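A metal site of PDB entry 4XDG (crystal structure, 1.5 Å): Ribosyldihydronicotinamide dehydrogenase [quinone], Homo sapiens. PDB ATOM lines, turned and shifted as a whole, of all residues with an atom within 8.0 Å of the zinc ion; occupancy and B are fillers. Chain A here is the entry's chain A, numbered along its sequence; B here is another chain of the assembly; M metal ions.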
ATOM      1  N   TYR A 133     -15.397   0.621  -0.726  1.00  0.00           N
ATOM      2  CA  TYR A 133     -14.208   1.259  -1.269  1.00  0.00           C
ATOM      3  C   TYR A 133     -14.058   0.885  -2.756  1.00  0.00           C
ATOM      4  O   TYR A 133     -14.866   1.352  -3.569  1.00  0.00           O
ATOM      5  CB  TYR A 133     -12.925   1.020  -0.437  1.00  0.00           C
ATOM      6  CG  TYR A 133     -12.875   1.858   0.819  1.00  0.00           C
ATOM      7  CD1 TYR A 133     -12.895   3.245   0.766  1.00  0.00           C
ATOM      8  CD2 TYR A 133     -12.754   1.259   2.074  1.00  0.00           C
ATOM      9  CE1 TYR A 133     -12.842   4.027   1.916  1.00  0.00           C
ATOM     10  CE2 TYR A 133     -12.683   2.031   3.243  1.00  0.00           C
ATOM     11  CZ  TYR A 133     -12.729   3.411   3.159  1.00  0.00           C
ATOM     12  OH  TYR A 133     -12.667   4.168   4.306  1.00  0.00           O
ATOM     13  N   ASP A 134     -13.121  -0.027  -3.105  1.00  0.00           N
ATOM     14  CA  ASP A 134     -12.994  -0.432  -4.515  1.00  0.00           C
ATOM     15  C   ASP A 134     -14.112  -1.398  -4.941  1.00  0.00           C
ATOM     16  O   ASP A 134     -14.340  -1.566  -6.148  1.00  0.00           O
ATOM     17  CB  ASP A 134     -11.594  -0.955  -4.848  1.00  0.00           C
ATOM     18  CG  ASP A 134     -10.474   0.054  -4.619  1.00  0.00           C
ATOM     19  OD1 ASP A 134     -10.778   1.272  -4.532  1.00  0.00           O
ATOM     20  OD2 ASP A 134      -9.309  -0.372  -4.501  1.00  0.00           O
ATOM     21  N   TRP A 170     -11.756  14.729   4.728  1.00  0.00           N
ATOM     22  CA  TRP A 170     -11.598  13.295   4.918  1.00  0.00           C
ATOM     23  C   TRP A 170     -12.920  12.524   5.114  1.00  0.00           C
ATOM     24  O   TRP A 170     -13.180  11.598   4.349  1.00  0.00           O
ATOM     25  CB  TRP A 170     -10.632  13.038   6.067  1.00  0.00           C
ATOM     26  CG  TRP A 170     -10.414  11.600   6.429  1.00  0.00           C
ATOM     27  CD1 TRP A 170     -10.806  10.979   7.586  1.00  0.00           C
ATOM     28  CD2 TRP A 170      -9.619  10.651   5.722  1.00  0.00           C
ATOM     29  NE1 TRP A 170     -10.332   9.690   7.614  1.00  0.00           N
ATOM     30  CE2 TRP A 170      -9.590   9.459   6.491  1.00  0.00           C
ATOM     31  CE3 TRP A 170      -8.925  10.679   4.485  1.00  0.00           C
ATOM     32  CZ2 TRP A 170      -8.898   8.316   6.074  1.00  0.00           C
ATOM     33  CZ3 TRP A 170      -8.242   9.539   4.079  1.00  0.00           C
ATOM     34  CH2 TRP A 170      -8.205   8.384   4.881  1.00  0.00           C
ATOM     35  N   LEU A 172     -15.918  13.216   4.202  1.00  0.00           N
ATOM     36  CA  LEU A 172     -16.757  13.394   3.016  1.00  0.00           C
ATOM     37  C   LEU A 172     -16.153  12.715   1.813  1.00  0.00           C
ATOM     38  O   LEU A 172     -16.807  11.882   1.195  1.00  0.00           O
ATOM     39  CB  LEU A 172     -16.964  14.895   2.741  1.00  0.00           C
ATOM     40  CG  LEU A 172     -17.632  15.702   3.867  1.00  0.00           C
ATOM     41  CD1 LEU A 172     -17.565  17.198   3.564  1.00  0.00           C
ATOM     42  CD2 LEU A 172     -19.102  15.274   4.038  1.00  0.00           C
ATOM     43  N   GLN A 173     -14.908  13.081   1.473  1.00  0.00           N
ATOM     44  CA  GLN A 173     -14.271  12.517   0.293  1.00  0.00           C
ATOM     45  C   GLN A 173     -13.938  11.056   0.472  1.00  0.00           C
ATOM     46  O   GLN A 173     -14.244  10.257  -0.441  1.00  0.00           O
ATOM     47  CB  GLN A 173     -13.001  13.288  -0.085  1.00  0.00           C
ATOM     48  CG  GLN A 173     -13.329  14.691  -0.562  1.00  0.00           C
ATOM     49  CD  GLN A 173     -12.132  15.435  -1.084  1.00  0.00           C
ATOM     50  OE1 GLN A 173     -10.933  15.156  -0.740  1.00  0.00           O
ATOM     51  NE2 GLN A 173     -12.400  16.435  -1.906  1.00  0.00           N
ATOM     52  N   HIS A 174     -13.319  10.698   1.617  1.00  0.00           N
ATOM     53  CA  HIS A 174     -12.881   9.317   1.826  1.00  0.00           C
ATOM     54  C   HIS A 174     -13.934   8.447   2.457  1.00  0.00           C
ATOM     55  O   HIS A 174     -14.289   7.420   1.901  1.00  0.00           O
ATOM     56  CB  HIS A 174     -11.561   9.255   2.607  1.00  0.00           C
ATOM     57  CG  HIS A 174     -10.996   7.868   2.716  1.00  0.00           C
ATOM     58  ND1 HIS A 174     -10.324   7.275   1.654  1.00  0.00           N
ATOM     59  CD2 HIS A 174     -11.007   7.010   3.761  1.00  0.00           C
ATOM     60  CE1 HIS A 174      -9.964   6.084   2.084  1.00  0.00           C
ATOM     61  NE2 HIS A 174     -10.329   5.883   3.356  1.00  0.00           N
ATOM     62  N   GLY A 175     -14.411   8.856   3.642  1.00  0.00           N
ATOM     63  CA  GLY A 175     -15.340   8.026   4.389  1.00  0.00           C
ATOM     64  C   GLY A 175     -16.684   7.820   3.710  1.00  0.00           C
ATOM     65  O   GLY A 175     -17.350   6.838   3.990  1.00  0.00           O
ATOM     66  N   THR A 176     -17.079   8.766   2.831  1.00  0.00           N
ATOM     67  CA  THR A 176     -18.376   8.683   2.145  1.00  0.00           C
ATOM     68  C   THR A 176     -18.237   8.401   0.678  1.00  0.00           C
ATOM     69  O   THR A 176     -18.624   7.324   0.208  1.00  0.00           O
ATOM     70  CB  THR A 176     -19.216   9.950   2.392  1.00  0.00           C
ATOM     71  OG1 THR A 176     -19.229  10.244   3.812  1.00  0.00           O
ATOM     72  CG2 THR A 176     -20.656   9.781   1.907  1.00  0.00           C
ATOM     73  N   LEU A 177     -17.681   9.355  -0.069  1.00  0.00           N
ATOM     74  CA  LEU A 177     -17.639   9.220  -1.541  1.00  0.00           C
ATOM     75  C   LEU A 177     -16.741   8.096  -2.014  1.00  0.00           C
ATOM     76  O   LEU A 177     -17.209   7.245  -2.773  1.00  0.00           O
ATOM     77  CB  LEU A 177     -17.284  10.560  -2.189  1.00  0.00           C
ATOM     78  CG  LEU A 177     -18.287  11.683  -1.849  1.00  0.00           C
ATOM     79  CD1 LEU A 177     -17.760  13.016  -2.274  1.00  0.00           C
ATOM     80  CD2 LEU A 177     -19.666  11.395  -2.436  1.00  0.00           C
ATOM     81  N   HIS A 178     -15.479   8.056  -1.583  1.00  0.00           N
ATOM     82  CA  HIS A 178     -14.583   6.968  -1.982  1.00  0.00           C
ATOM     83  C   HIS A 178     -15.151   5.637  -1.496  1.00  0.00           C
ATOM     84  O   HIS A 178     -15.093   4.656  -2.244  1.00  0.00           O
ATOM     85  CB  HIS A 178     -13.171   7.212  -1.439  1.00  0.00           C
ATOM     86  CG  HIS A 178     -12.106   6.252  -1.902  1.00  0.00           C
ATOM     87  ND1 HIS A 178     -10.803   6.367  -1.445  1.00  0.00           N
ATOM     88  CD2 HIS A 178     -12.163   5.255  -2.814  1.00  0.00           C
ATOM     89  CE1 HIS A 178     -10.121   5.405  -2.043  1.00  0.00           C
ATOM     90  NE2 HIS A 178     -10.891   4.695  -2.861  1.00  0.00           N
ATOM     91  N   PHE A 179     -15.693   5.604  -0.268  1.00  0.00           N
ATOM     92  CA  PHE A 179     -16.255   4.376   0.269  1.00  0.00           C
ATOM     93  C   PHE A 179     -17.311   3.794  -0.668  1.00  0.00           C
ATOM     94  O   PHE A 179     -17.359   2.587  -0.828  1.00  0.00           O
ATOM     95  CB  PHE A 179     -16.817   4.613   1.657  1.00  0.00           C
ATOM     96  CG  PHE A 179     -17.228   3.357   2.393  1.00  0.00           C
ATOM     97  CD1 PHE A 179     -16.322   2.678   3.195  1.00  0.00           C
ATOM     98  CD2 PHE A 179     -18.539   2.890   2.320  1.00  0.00           C
ATOM     99  CE1 PHE A 179     -16.713   1.538   3.904  1.00  0.00           C
ATOM    100  CE2 PHE A 179     -18.925   1.758   3.041  1.00  0.00           C
ATOM    101  CZ  PHE A 179     -18.015   1.110   3.845  1.00  0.00           C
ATOM    102  N   PHE A 182     -17.002   6.156  -5.683  1.00  0.00           N
ATOM    103  CA  PHE A 182     -16.749   7.319  -6.512  1.00  0.00           C
ATOM    104  C   PHE A 182     -15.240   7.591  -6.639  1.00  0.00           C
ATOM    105  O   PHE A 182     -14.460   7.359  -5.710  1.00  0.00           O
ATOM    106  CB  PHE A 182     -17.343   8.581  -5.881  1.00  0.00           C
ATOM    107  CG  PHE A 182     -18.835   8.779  -5.935  1.00  0.00           C
ATOM    108  CD1 PHE A 182     -19.439   9.306  -7.062  1.00  0.00           C
ATOM    109  CD2 PHE A 182     -19.626   8.511  -4.825  1.00  0.00           C
ATOM    110  CE1 PHE A 182     -20.820   9.526  -7.103  1.00  0.00           C
ATOM    111  CE2 PHE A 182     -21.003   8.739  -4.855  1.00  0.00           C
ATOM    112  CZ  PHE A 182     -21.589   9.259  -5.992  1.00  0.00           C
ATOM    113  N   VAL A 184     -12.982  10.830  -6.914  1.00  0.00           N
ATOM    114  CA  VAL A 184     -13.191  12.163  -6.372  1.00  0.00           C
ATOM    115  C   VAL A 184     -12.387  13.197  -7.109  1.00  0.00           C
ATOM    116  O   VAL A 184     -11.169  13.128  -7.134  1.00  0.00           O
ATOM    117  CB  VAL A 184     -12.848  12.173  -4.839  1.00  0.00           C
ATOM    118  CG1 VAL A 184     -12.992  13.567  -4.229  1.00  0.00           C
ATOM    119  CG2 VAL A 184     -13.706  11.164  -4.090  1.00  0.00           C
ATOM    120  N   ILE A 221      -8.433  12.875  -7.726  1.00  0.00           N
ATOM    121  CA  ILE A 221      -7.336  12.934  -6.774  1.00  0.00           C
ATOM    122  C   ILE A 221      -7.048  11.517  -6.298  1.00  0.00           C
ATOM    123  O   ILE A 221      -7.931  10.643  -6.360  1.00  0.00           O
ATOM    124  CB  ILE A 221      -7.702  13.831  -5.545  1.00  0.00           C
ATOM    125  CG1 ILE A 221      -8.887  13.226  -4.727  1.00  0.00           C
ATOM    126  CG2 ILE A 221      -7.938  15.280  -5.936  1.00  0.00           C
ATOM    127  CD1 ILE A 221      -9.069  13.747  -3.315  1.00  0.00           C
ATOM    128  N   PRO A 222      -5.838  11.265  -5.740  1.00  0.00           N
ATOM    129  CA  PRO A 222      -5.618   9.990  -5.049  1.00  0.00           C
ATOM    130  C   PRO A 222      -6.246  10.158  -3.659  1.00  0.00           C
ATOM    131  O   PRO A 222      -5.741  10.917  -2.839  1.00  0.00           O
ATOM    132  CB  PRO A 222      -4.086   9.876  -5.015  1.00  0.00           C
ATOM    133  CG  PRO A 222      -3.569  11.298  -5.100  1.00  0.00           C
ATOM    134  CD  PRO A 222      -4.679  12.179  -5.630  1.00  0.00           C
ATOM    135  N   CYS A 223      -7.423   9.574  -3.452  1.00  0.00           N
ATOM    136  CA  CYS A 223      -8.175   9.774  -2.211  1.00  0.00           C
ATOM    137  C   CYS A 223      -7.637   8.900  -1.092  1.00  0.00           C
ATOM    138  O   CYS A 223      -8.204   7.862  -0.736  1.00  0.00           O
ATOM    139  CB  CYS A 223      -9.663   9.578  -2.458  1.00  0.00           C
ATOM    140  SG  CYS A 223     -10.676   9.981  -1.018  1.00  0.00           S
ATOM    141  N   THR A 224      -6.451   9.302  -0.595  1.00  0.00           N
ATOM    142  CA  THR A 224      -5.721   8.582   0.422  1.00  0.00           C
ATOM    143  C   THR A 224      -5.451   9.443   1.643  1.00  0.00           C
ATOM    144  O   THR A 224      -5.557  10.672   1.572  1.00  0.00           O
ATOM    145  CB  THR A 224      -4.356   8.174  -0.191  1.00  0.00           C
ATOM    146  OG1 THR A 224      -3.613   9.366  -0.479  1.00  0.00           O
ATOM    147  CG2 THR A 224      -4.486   7.305  -1.431  1.00  0.00           C
ATOM    148  N   ALA A 225      -5.020   8.812   2.747  1.00  0.00           N
ATOM    149  CA  ALA A 225      -4.649   9.559   3.947  1.00  0.00           C
ATOM    150  C   ALA A 225      -3.463  10.497   3.626  1.00  0.00           C
ATOM    151  O   ALA A 225      -3.422  11.612   4.148  1.00  0.00           O
ATOM    152  CB  ALA A 225      -4.252   8.597   5.065  1.00  0.00           C
ATOM    153  N   TRP A 227      -2.805  12.104   0.777  1.00  0.00           N
ATOM    154  CA  TRP A 227      -3.319  13.294   0.114  1.00  0.00           C
ATOM    155  C   TRP A 227      -3.939  14.259   1.126  1.00  0.00           C
ATOM    156  O   TRP A 227      -3.682  15.456   1.075  1.00  0.00           O
ATOM    157  CB  TRP A 227      -4.346  12.926  -0.961  1.00  0.00           C
ATOM    158  CG  TRP A 227      -4.791  14.089  -1.787  1.00  0.00           C
ATOM    159  CD1 TRP A 227      -4.234  14.521  -2.952  1.00  0.00           C
ATOM    160  CD2 TRP A 227      -5.884  14.982  -1.502  1.00  0.00           C
ATOM    161  NE1 TRP A 227      -4.910  15.611  -3.426  1.00  0.00           N
ATOM    162  CE2 TRP A 227      -5.923  15.922  -2.559  1.00  0.00           C
ATOM    163  CE3 TRP A 227      -6.824  15.084  -0.465  1.00  0.00           C
ATOM    164  CZ2 TRP A 227      -6.885  16.936  -2.621  1.00  0.00           C
ATOM    165  CZ3 TRP A 227      -7.759  16.105  -0.506  1.00  0.00           C
ATOM    166  CH2 TRP A 227      -7.789  17.020  -1.585  1.00  0.00           C
ATOM    167  N   HIS A 228      -4.724  13.736   2.088  1.00  0.00           N
ATOM    168  CA  HIS A 228      -5.412  14.584   3.047  1.00  0.00           C
ATOM    169  C   HIS A 228      -4.523  15.127   4.149  1.00  0.00           C
ATOM    170  O   HIS A 228      -4.705  16.267   4.601  1.00  0.00           O
ATOM    171  CB  HIS A 228      -6.601  13.846   3.680  1.00  0.00           C
ATOM    172  CG  HIS A 228      -7.734  13.572   2.714  1.00  0.00           C
ATOM    173  ND1 HIS A 228      -7.700  12.507   1.816  1.00  0.00           N
ATOM    174  CD2 HIS A 228      -8.916  14.221   2.570  1.00  0.00           C
ATOM    175  CE1 HIS A 228      -8.842  12.562   1.137  1.00  0.00           C
ATOM    176  NE2 HIS A 228      -9.612  13.563   1.568  1.00  0.00           N
ATOM    177  N   VAL B 161      -7.897   0.418   6.328  1.00  0.00           N
ATOM    178  CA  VAL B 161      -8.613   0.967   5.183  1.00  0.00           C
ATOM    179  C   VAL B 161      -9.378   2.268   5.505  1.00  0.00           C
ATOM    180  O   VAL B 161      -9.557   3.131   4.629  1.00  0.00           O
ATOM    181  CB  VAL B 161      -9.503  -0.131   4.564  1.00  0.00           C
ATOM    182  CG1 VAL B 161     -10.800  -0.362   5.320  1.00  0.00           C
ATOM    183  CG2 VAL B 161      -9.690   0.089   3.097  1.00  0.00           C
HETATM  184 ZN    ZN M   1     -10.202   7.927  -0.226  1.00  0.00          ZN
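NE2 of His 174 lies within hydrogen-bond range of O of Val 161 of chain B (3.1 Å). O of His 174 is in hydrogen-bond range of N of Phe 179. SG of Cys 223 sits close to O of Gln 173, at 3.6 Å. The backbone NH (N) of His 178 lies within hydrogen-bond range of the backbone carbonyl oxygen (O) of Gln 173, at 2.8 Å. A ring nitrogen (NE2) of His 174 lies within hydrogen-bond range of the side-chain hydroxyl (OH) of Tyr 133.
The zinc ion is bound by ND1 of His 174 (2.0 Å). O of Cys 223 is bound to the zinc ion, 2.1 Å away. ND1 of His 178 binds the zinc ion, 2.1 Å away. The zinc ion is bound by SG of Cys 223.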
